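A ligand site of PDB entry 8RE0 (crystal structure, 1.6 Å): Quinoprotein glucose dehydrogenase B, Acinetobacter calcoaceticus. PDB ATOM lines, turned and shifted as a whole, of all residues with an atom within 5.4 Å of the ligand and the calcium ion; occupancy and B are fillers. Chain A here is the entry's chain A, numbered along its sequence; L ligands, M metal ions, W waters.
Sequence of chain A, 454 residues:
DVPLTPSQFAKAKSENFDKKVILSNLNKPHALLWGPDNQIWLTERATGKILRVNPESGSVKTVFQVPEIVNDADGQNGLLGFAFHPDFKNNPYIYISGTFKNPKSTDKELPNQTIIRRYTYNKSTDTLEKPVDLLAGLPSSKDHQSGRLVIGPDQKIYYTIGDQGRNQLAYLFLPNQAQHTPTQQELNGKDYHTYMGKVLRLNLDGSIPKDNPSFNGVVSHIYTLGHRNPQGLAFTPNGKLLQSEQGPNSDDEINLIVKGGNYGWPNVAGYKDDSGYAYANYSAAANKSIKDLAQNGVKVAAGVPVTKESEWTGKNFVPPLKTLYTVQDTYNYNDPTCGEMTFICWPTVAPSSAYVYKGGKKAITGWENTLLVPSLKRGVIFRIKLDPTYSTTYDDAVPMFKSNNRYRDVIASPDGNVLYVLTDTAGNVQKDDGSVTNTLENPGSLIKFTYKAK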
ATOM      1  N   GLN A  76      19.833   9.410 -10.740  1.00  0.00           N
ATOM      2  CA  GLN A  76      19.912   8.418  -9.686  1.00  0.00           C
ATOM      3  C   GLN A  76      19.974   9.070  -8.305  1.00  0.00           C
ATOM      4  O   GLN A  76      20.417   8.446  -7.338  1.00  0.00           O
ATOM      5  CB  GLN A  76      21.141   7.550  -9.916  1.00  0.00           C
ATOM      6  CG  GLN A  76      21.031   6.655 -11.110  1.00  0.00           C
ATOM      7  CD  GLN A  76      21.974   7.078 -12.218  1.00  0.00           C
ATOM      8  OE1 GLN A  76      21.662   8.001 -12.991  1.00  0.00           O
ATOM      9  NE2 GLN A  76      23.187   6.461 -12.246  1.00  0.00           N
ATOM     10  N   HIS A 144      25.921   8.284 -10.483  1.00  0.00           N
ATOM     11  CA  HIS A 144      26.893   7.604  -9.615  1.00  0.00           C
ATOM     12  C   HIS A 144      26.923   8.260  -8.241  1.00  0.00           C
ATOM     13  O   HIS A 144      27.952   8.741  -7.759  1.00  0.00           O
ATOM     14  CB  HIS A 144      28.322   7.559 -10.197  1.00  0.00           C
ATOM     15  CG  HIS A 144      28.399   7.005 -11.589  1.00  0.00           C
ATOM     16  ND1 HIS A 144      29.537   7.092 -12.365  1.00  0.00           N
ATOM     17  CD2 HIS A 144      27.500   6.321 -12.330  1.00  0.00           C
ATOM     18  CE1 HIS A 144      29.315   6.547 -13.548  1.00  0.00           C
ATOM     19  NE2 HIS A 144      28.078   6.067 -13.545  1.00  0.00           N
ATOM     20  N   ARG A 228      34.181   4.175  -8.203  1.00  0.00           N
ATOM     21  CA  ARG A 228      33.325   4.726  -9.253  1.00  0.00           C
ATOM     22  C   ARG A 228      31.890   4.834  -8.727  1.00  0.00           C
ATOM     23  O   ARG A 228      31.453   5.912  -8.321  1.00  0.00           O
ATOM     24  CB  ARG A 228      33.432   3.868 -10.523  1.00  0.00           C
ATOM     25  CG  ARG A 228      32.672   4.400 -11.692  1.00  0.00           C
ATOM     26  CD  ARG A 228      32.757   3.426 -12.899  1.00  0.00           C
ATOM     27  NE  ARG A 228      31.957   3.856 -14.046  1.00  0.00           N
ATOM     28  CZ  ARG A 228      30.663   3.588 -14.197  1.00  0.00           C
ATOM     29  NH1 ARG A 228      29.986   2.937 -13.278  1.00  0.00           N
ATOM     30  NH2 ARG A 228      30.032   3.948 -15.315  1.00  0.00           N
ATOM     31  N   ASN A 229      31.158   3.732  -8.682  1.00  0.00           N
ATOM     32  CA  ASN A 229      29.784   3.741  -8.163  1.00  0.00           C
ATOM     33  C   ASN A 229      29.599   2.536  -7.246  1.00  0.00           C
ATOM     34  O   ASN A 229      29.007   1.510  -7.614  1.00  0.00           O
ATOM     35  CB  ASN A 229      28.743   3.765  -9.292  1.00  0.00           C
ATOM     36  CG  ASN A 229      27.318   3.914  -8.769  1.00  0.00           C
ATOM     37  OD1 ASN A 229      27.125   4.312  -7.624  1.00  0.00           O
ATOM     38  ND2 ASN A 229      26.334   3.600  -9.593  1.00  0.00           N
ATOM     39  N   GLN A 231      27.634   0.733  -4.891  1.00  0.00           N
ATOM     40  CA  GLN A 231      26.292   0.687  -4.320  1.00  0.00           C
ATOM     41  C   GLN A 231      26.087  -0.415  -3.299  1.00  0.00           C
ATOM     42  O   GLN A 231      25.052  -0.421  -2.630  1.00  0.00           O
ATOM     43  CB  GLN A 231      25.259   0.507  -5.432  1.00  0.00           C
ATOM     44  CG  GLN A 231      25.136   1.706  -6.379  1.00  0.00           C
ATOM     45  CD  GLN A 231      24.108   1.490  -7.479  1.00  0.00           C
ATOM     46  OE1 GLN A 231      23.811   0.360  -7.848  1.00  0.00           O
ATOM     47  NE2 GLN A 231      23.555   2.572  -7.979  1.00  0.00           N
ATOM     48  N   GLN A 246      29.945  -0.631  -9.422  1.00  0.00           N
ATOM     49  CA  GLN A 246      29.736  -0.663 -10.861  1.00  0.00           C
ATOM     50  C   GLN A 246      30.949  -0.064 -11.577  1.00  0.00           C
ATOM     51  O   GLN A 246      31.340   1.085 -11.299  1.00  0.00           O
ATOM     52  CB  GLN A 246      28.457   0.090 -11.251  1.00  0.00           C
ATOM     53  CG  GLN A 246      27.208  -0.419 -10.590  1.00  0.00           C
ATOM     54  CD  GLN A 246      25.932  -0.064 -11.320  1.00  0.00           C
ATOM     55  OE1 GLN A 246      25.943   0.176 -12.512  1.00  0.00           O
ATOM     56  NE2 GLN A 246      24.826  -0.017 -10.599  1.00  0.00           N
ATOM     57  N   GLY A 247      31.498  -0.820 -12.525  1.00  0.00           N
ATOM     58  CA  GLY A 247      32.510  -0.327 -13.444  1.00  0.00           C
ATOM     59  C   GLY A 247      31.877   0.242 -14.700  1.00  0.00           C
ATOM     60  O   GLY A 247      30.651   0.324 -14.837  1.00  0.00           O
ATOM     61  N   PRO A 248      32.730   0.711 -15.631  1.00  0.00           N
ATOM     62  CA  PRO A 248      32.232   1.325 -16.884  1.00  0.00           C
ATOM     63  C   PRO A 248      31.699   0.308 -17.885  1.00  0.00           C
ATOM     64  O   PRO A 248      30.626  -0.253 -17.620  1.00  0.00           O
ATOM     65  CB  PRO A 248      33.451   2.108 -17.384  1.00  0.00           C
ATOM     66  CG  PRO A 248      34.617   1.178 -16.978  1.00  0.00           C
ATOM     67  CD  PRO A 248      34.210   0.716 -15.567  1.00  0.00           C
ATOM     68  N   ASN A 249      32.357   0.091 -19.031  1.00  0.00           N
ATOM     69  CA  ASN A 249      31.882  -0.954 -19.944  1.00  0.00           C
ATOM     70  C   ASN A 249      32.256  -2.356 -19.479  1.00  0.00           C
ATOM     71  O   ASN A 249      31.883  -3.340 -20.136  1.00  0.00           O
ATOM     72  CB  ASN A 249      32.412  -0.839 -21.368  1.00  0.00           C
ATOM     73  CG  ASN A 249      32.185   0.498 -22.014  1.00  0.00           C
ATOM     74  OD1 ASN A 249      31.836   1.482 -21.386  1.00  0.00           O
ATOM     75  ND2 ASN A 249      32.378   0.531 -23.306  1.00  0.00           N
ATOM     76  N   ASP A 252      32.830  -4.472 -13.347  1.00  0.00           N
ATOM     77  CA  ASP A 252      32.153  -4.395 -12.056  1.00  0.00           C
ATOM     78  C   ASP A 252      32.997  -5.161 -11.056  1.00  0.00           C
ATOM     79  O   ASP A 252      33.701  -6.119 -11.418  1.00  0.00           O
ATOM     80  CB  ASP A 252      30.747  -4.979 -12.119  1.00  0.00           C
ATOM     81  CG  ASP A 252      29.830  -4.182 -13.083  1.00  0.00           C
ATOM     82  OD1 ASP A 252      29.937  -2.954 -13.198  1.00  0.00           O
ATOM     83  OD2 ASP A 252      28.912  -4.817 -13.614  1.00  0.00           O
ATOM     84  N   PHE A 343      25.210  -2.285 -25.794  1.00  0.00           N
ATOM     85  CA  PHE A 343      25.582  -2.216 -24.395  1.00  0.00           C
ATOM     86  C   PHE A 343      25.054  -3.398 -23.587  1.00  0.00           C
ATOM     87  O   PHE A 343      25.612  -3.719 -22.536  1.00  0.00           O
ATOM     88  CB  PHE A 343      25.062  -0.903 -23.809  1.00  0.00           C
ATOM     89  CG  PHE A 343      23.628  -0.968 -23.308  1.00  0.00           C
ATOM     90  CD1 PHE A 343      23.333  -1.521 -22.072  1.00  0.00           C
ATOM     91  CD2 PHE A 343      22.595  -0.482 -24.084  1.00  0.00           C
ATOM     92  CE1 PHE A 343      22.030  -1.590 -21.614  1.00  0.00           C
ATOM     93  CE2 PHE A 343      21.290  -0.552 -23.636  1.00  0.00           C
ATOM     94  CZ  PHE A 343      21.010  -1.101 -22.402  1.00  0.00           C
ATOM     95  N   TRP A 346      27.643  -5.955 -23.043  1.00  0.00           N
ATOM     96  CA  TRP A 346      28.891  -5.521 -22.427  1.00  0.00           C
ATOM     97  C   TRP A 346      29.211  -6.450 -21.250  1.00  0.00           C
ATOM     98  O   TRP A 346      28.283  -6.967 -20.610  1.00  0.00           O
ATOM     99  CB  TRP A 346      28.794  -4.075 -21.945  1.00  0.00           C
ATOM    100  CG  TRP A 346      28.929  -3.081 -23.021  1.00  0.00           C
ATOM    101  CD1 TRP A 346      29.132  -3.307 -24.353  1.00  0.00           C
ATOM    102  CD2 TRP A 346      28.858  -1.658 -22.862  1.00  0.00           C
ATOM    103  NE1 TRP A 346      29.212  -2.116 -25.016  1.00  0.00           N
ATOM    104  CE2 TRP A 346      29.046  -1.089 -24.129  1.00  0.00           C
ATOM    105  CE3 TRP A 346      28.661  -0.824 -21.773  1.00  0.00           C
ATOM    106  CZ2 TRP A 346      29.028   0.280 -24.344  1.00  0.00           C
ATOM    107  CZ3 TRP A 346      28.635   0.550 -21.978  1.00  0.00           C
ATOM    108  CH2 TRP A 346      28.826   1.083 -23.252  1.00  0.00           C
ATOM    109  N   THR A 348      29.476  -6.625 -18.126  1.00  0.00           N
ATOM    110  CA  THR A 348      29.119  -6.057 -16.837  1.00  0.00           C
ATOM    111  C   THR A 348      27.813  -6.700 -16.381  1.00  0.00           C
ATOM    112  O   THR A 348      27.077  -7.325 -17.162  1.00  0.00           O
ATOM    113  CB  THR A 348      28.921  -4.547 -16.935  1.00  0.00           C
ATOM    114  OG1 THR A 348      28.000  -4.272 -18.017  1.00  0.00           O
ATOM    115  CG2 THR A 348      30.263  -3.859 -17.177  1.00  0.00           C
ATOM    116  N   ALA A 350      26.125  -4.723 -13.587  1.00  0.00           N
ATOM    117  CA  ALA A 350      25.561  -3.575 -12.882  1.00  0.00           C
ATOM    118  C   ALA A 350      25.050  -3.976 -11.496  1.00  0.00           C
ATOM    119  O   ALA A 350      23.829  -3.947 -11.256  1.00  0.00           O
ATOM    120  CB  ALA A 350      24.436  -2.936 -13.702  1.00  0.00           C
ATOM    121  N   LEU A 376      21.243  -5.453 -11.870  1.00  0.00           N
ATOM    122  CA  LEU A 376      20.221  -4.692 -12.569  1.00  0.00           C
ATOM    123  C   LEU A 376      20.079  -5.164 -14.008  1.00  0.00           C
ATOM    124  O   LEU A 376      18.972  -5.403 -14.493  1.00  0.00           O
ATOM    125  CB  LEU A 376      20.550  -3.203 -12.516  1.00  0.00           C
ATOM    126  CG  LEU A 376      20.604  -2.569 -11.133  1.00  0.00           C
ATOM    127  CD1 LEU A 376      21.307  -1.211 -11.228  1.00  0.00           C
ATOM    128  CD2 LEU A 376      19.219  -2.413 -10.565  1.00  0.00           C
ATOM    129  N   LYS A 377      21.201  -5.316 -14.691  1.00  0.00           N
ATOM    130  CA  LYS A 377      21.205  -5.501 -16.128  1.00  0.00           C
ATOM    131  C   LYS A 377      20.890  -6.922 -16.552  1.00  0.00           C
ATOM    132  O   LYS A 377      20.337  -7.138 -17.628  1.00  0.00           O
ATOM    133  CB  LYS A 377      22.575  -5.074 -16.694  1.00  0.00           C
ATOM    134  CG  LYS A 377      22.782  -5.298 -18.168  1.00  0.00           C
ATOM    135  CD  LYS A 377      24.100  -4.658 -18.605  1.00  0.00           C
ATOM    136  CE  LYS A 377      25.079  -5.675 -19.121  1.00  0.00           C
ATOM    137  NZ  LYS A 377      26.171  -5.005 -19.851  1.00  0.00           N
ATOM    138  N   ARG A 406      14.901  -5.735 -12.981  1.00  0.00           N
ATOM    139  CA  ARG A 406      16.113  -5.069 -12.533  1.00  0.00           C
ATOM    140  C   ARG A 406      16.131  -5.200 -11.011  1.00  0.00           C
ATOM    141  O   ARG A 406      15.423  -4.463 -10.297  1.00  0.00           O
ATOM    142  CB  ARG A 406      16.088  -3.624 -12.965  1.00  0.00           C
ATOM    143  CG  ARG A 406      16.461  -3.420 -14.401  1.00  0.00           C
ATOM    144  CD  ARG A 406      16.043  -2.016 -14.852  1.00  0.00           C
ATOM    145  NE  ARG A 406      16.929  -1.037 -14.226  1.00  0.00           N
ATOM    146  CZ  ARG A 406      18.180  -0.796 -14.613  1.00  0.00           C
ATOM    147  NH1 ARG A 406      18.742  -1.432 -15.623  1.00  0.00           N
ATOM    148  NH2 ARG A 406      18.899   0.093 -13.943  1.00  0.00           N
ATOM    149  N   ARG A 408      17.303  -4.648  -7.382  1.00  0.00           N
ATOM    150  CA  ARG A 408      17.844  -3.441  -6.782  1.00  0.00           C
ATOM    151  C   ARG A 408      18.418  -3.680  -5.396  1.00  0.00           C
ATOM    152  O   ARG A 408      19.340  -2.978  -5.013  1.00  0.00           O
ATOM    153  CB  ARG A 408      16.752  -2.351  -6.725  1.00  0.00           C
ATOM    154  CG  ARG A 408      17.119  -1.077  -6.032  1.00  0.00           C
ATOM    155  CD  ARG A 408      18.286  -0.299  -6.598  1.00  0.00           C
ATOM    156  NE  ARG A 408      18.140   0.094  -7.998  1.00  0.00           N
ATOM    157  CZ  ARG A 408      19.090   0.665  -8.736  1.00  0.00           C
ATOM    158  NH1 ARG A 408      20.281   0.978  -8.225  1.00  0.00           N
ATOM    159  NH2 ARG A 408      18.821   1.003  -9.998  1.00  0.00           N
ATOM    160  N   ASP A 424      13.392  -2.493  -9.758  1.00  0.00           N
ATOM    161  CA  ASP A 424      13.262  -1.138 -10.243  1.00  0.00           C
ATOM    162  C   ASP A 424      11.896  -0.942 -10.900  1.00  0.00           C
ATOM    163  O   ASP A 424      11.271  -1.888 -11.383  1.00  0.00           O
ATOM    164  CB  ASP A 424      14.346  -0.821 -11.275  1.00  0.00           C
ATOM    165  CG  ASP A 424      15.648  -0.392 -10.654  1.00  0.00           C
ATOM    166  OD1 ASP A 424      15.777  -0.322  -9.402  1.00  0.00           O
ATOM    167  OD2 ASP A 424      16.548  -0.086 -11.455  1.00  0.00           O
ATOM    168  N   ASN A 428      16.255  -0.916 -18.536  1.00  0.00           N
ATOM    169  CA  ASN A 428      16.558  -2.027 -19.440  1.00  0.00           C
ATOM    170  C   ASN A 428      17.067  -3.243 -18.682  1.00  0.00           C
ATOM    171  O   ASN A 428      17.723  -3.131 -17.647  1.00  0.00           O
ATOM    172  CB  ASN A 428      17.602  -1.612 -20.477  1.00  0.00           C
ATOM    173  CG  ASN A 428      17.191  -0.378 -21.246  1.00  0.00           C
ATOM    174  OD1 ASN A 428      16.094  -0.328 -21.807  1.00  0.00           O
ATOM    175  ND2 ASN A 428      18.060   0.636 -21.257  1.00  0.00           N
HETATM  176  C1  LIG L   1      23.444   0.021 -16.335  1.00  0.00           C
HETATM  177  C2  LIG L   1      24.169  -0.799 -17.184  1.00  0.00           C
HETATM  178  C3  LIG L   1      25.556  -0.686 -17.170  1.00  0.00           C
HETATM  179  C4  LIG L   1      25.503   0.989 -15.582  1.00  0.00           C
HETATM  180  C5  LIG L   1      23.288   1.837 -14.678  1.00  0.00           C
HETATM  181  C6  LIG L   1      21.796   3.309 -13.797  1.00  0.00           C
HETATM  182  C7  LIG L   1      22.171   3.484 -16.360  1.00  0.00           C
HETATM  183  C8  LIG L   1      26.357   1.924 -14.738  1.00  0.00           C
HETATM  184  C9  LIG L   1      26.406  -1.586 -18.056  1.00  0.00           C
HETATM  185  C10 LIG L   1      22.265   2.509 -12.777  1.00  0.00           C
HETATM  186  C11 LIG L   1      22.428   2.894 -15.004  1.00  0.00           C
HETATM  187  C12 LIG L   1      21.923   2.474 -11.308  1.00  0.00           C
HETATM  188  C13 LIG L   1      21.955  -0.166 -16.282  1.00  0.00           C
HETATM  189  C14 LIG L   1      24.094   0.955 -15.510  1.00  0.00           C
HETATM  190  N1  LIG L   1      23.176   1.625 -13.317  1.00  0.00           N
HETATM  191  N2  LIG L   1      26.209   0.195 -16.392  1.00  0.00           N
HETATM  192  O1  LIG L   1      21.324  -0.117 -17.363  1.00  0.00           O
HETATM  193  O2  LIG L   1      21.179   4.240 -16.487  1.00  0.00           O
HETATM  194  O3  LIG L   1      22.970   3.169 -17.290  1.00  0.00           O
HETATM  195  O4  LIG L   1      20.872   3.019 -10.958  1.00  0.00           O
HETATM  196  O5  LIG L   1      22.706   1.899 -10.541  1.00  0.00           O
HETATM  197  O6  LIG L   1      25.761   2.870 -14.144  1.00  0.00           O
HETATM  198  O7  LIG L   1      27.614   1.696 -14.722  1.00  0.00           O
HETATM  199  O8  LIG L   1      25.814  -2.272 -18.917  1.00  0.00           O
HETATM  200  O9  LIG L   1      27.648  -1.578 -17.857  1.00  0.00           O
HETATM  201  O10 LIG L   1      21.434  -0.339 -15.166  1.00  0.00           O
HETATM  202 CA    CA M   1      28.640   0.046 -16.238  1.00  0.00          CA
HETATM  203  O   HOH W   1      19.298   4.300  -8.792  1.00  0.00           O
HETATM  204  O   HOH W   2      18.689   0.925 -17.683  1.00  0.00           O
HETATM  205  O   HOH W   3      28.090  -1.642 -14.588  1.00  0.00           O
HETATM  206  O   HOH W   4      20.634  -2.715 -18.123  1.00  0.00           O
HETATM  207  O   HOH W   5      18.555   3.156 -15.620  1.00  0.00           O
HETATM  208  O   HOH W   6      28.363   1.995 -17.555  1.00  0.00           O
HETATM  209  O   HOH W   7      26.128   3.485 -17.661  1.00  0.00           O
HETATM  210  O   HOH W   8      24.017   5.703 -18.426  1.00  0.00           O
HETATM  211  O   HOH W   9      18.317   2.776 -12.559  1.00  0.00           O
HETATM  212  O   HOH W  10      27.173   4.777 -15.878  1.00  0.00           O
HETATM  213  O   HOH W  11      25.220   5.506 -14.626  1.00  0.00           O
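Residues that only touch the ligand: Gln 76 (3.6 Å), His 144 (3.99 Å), Phe 343 (3.9 Å) and Leu 376 (3.5 Å).
Within 4 Å of the ligand: Gln 76, His 144, Arg 228, Gln 231, Gln 246, Gly 247, Pro 248, Phe 343, Thr 348, Leu 376, Lys 377, Arg 406 and Arg 408.
Two residues have an atom within 4 Å of the calcium ion: Gly 247 and Pro 248.
The guanidinium group of Arg 228 lies close to a ring nitrogen (NE2) of His 144, 3.4 Å away.
N of Leu 376 lies within hydrogen-bond range of O of Ala 350 (3.1 Å).
NH1 of Arg 406 is in hydrogen-bond range of O of Asn 428, at 2.8 Å.
ND2 of Asn 229 lies close to NE2 of Gln 231, 3.4 Å away.
The backbone carbonyl oxygen (O) of Gly 247 lies close to the guanidinium group (NH1) of Arg 228, at 3.1 Å.
NZ of Lys 377 is in hydrogen-bond range of O of Trp 346, at 3.0 Å.
OD1 of Asp 252 lies within hydrogen-bond range of N of Gly 247 (2.7 Å).
The side-chain hydroxyl of Thr 348 sits at hydrogen-bond distance from the side-chain amino group of Lys 377 (2.7 Å).
The calcium ion is bound by water W6 (2.4 Å), water W3 (2.4 Å), O of Pro 248 (2.4 Å), N2 of the ligand (2.4 Å), O7 of the ligand (2.5 Å), O of Gly 247 (2.5 Å) and O9 of the ligand (2.5 Å).
The calcium ion has seven donor atoms within binding distance.
Water W3 bridges the side-chain carboxylate of Asp 252 (2.7 Å) and the side-chain amide oxygen of Gln 246 (3.5 Å).
Water W11 lies within hydrogen-bond range of O6 of the ligand, NE2 of His 144 and NE2 of Gln 76.
Water W4 lies within hydrogen-bond range of an oxygen (O1) of the ligand, the backbone carbonyl oxygen (O) of Asn 428 and the guanidinium group (NH1) of Arg 406.
Water W2 lies within hydrogen-bond range of an oxygen (O1) of the ligand (2.9 Å), the guanidinium group of Arg 406 (3.1 Å) and the backbone NH of Asn 428 (3.2 Å).
Water W10 lies within hydrogen-bond range of a ring nitrogen (NE2) of His 144 (2.8 Å), an oxygen (O6) of the ligand (2.9 Å) and the guanidinium group of Arg 228 (3.0 Å).
Water W9 lies within hydrogen-bond range of O4 of the ligand (3.0 Å), NH2 of Arg 406 (3.1 Å) and NH2 of Arg 408 (3.2 Å).
O5 of the ligand sits at hydrogen-bond distance from NE2 of Gln 231.
An oxygen (O8) of the ligand is in salt-bridge range of the side-chain amino group of Lys 377 (2.9 Å).
The guanidinium group of Arg 406 lies within salt-bridge range of an oxygen (O10) of the ligand, 2.8 Å away.
The side-chain amide nitrogen (NE2) of Gln 246 is in hydrogen-bond range of an oxygen (O5) of the ligand (2.9 Å).
An oxygen (O8) of the ligand lies within hydrogen-bond range of the side-chain hydroxyl (OG1) of Thr 348 (3.1 Å).
An oxygen (O7) of the ligand sits close to the guanidinium group (NH1) of Arg 228 (3.0 Å).
The guanidinium group of Arg 408 lies within salt-bridge range of an oxygen (O4) of the ligand (3.0 Å).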
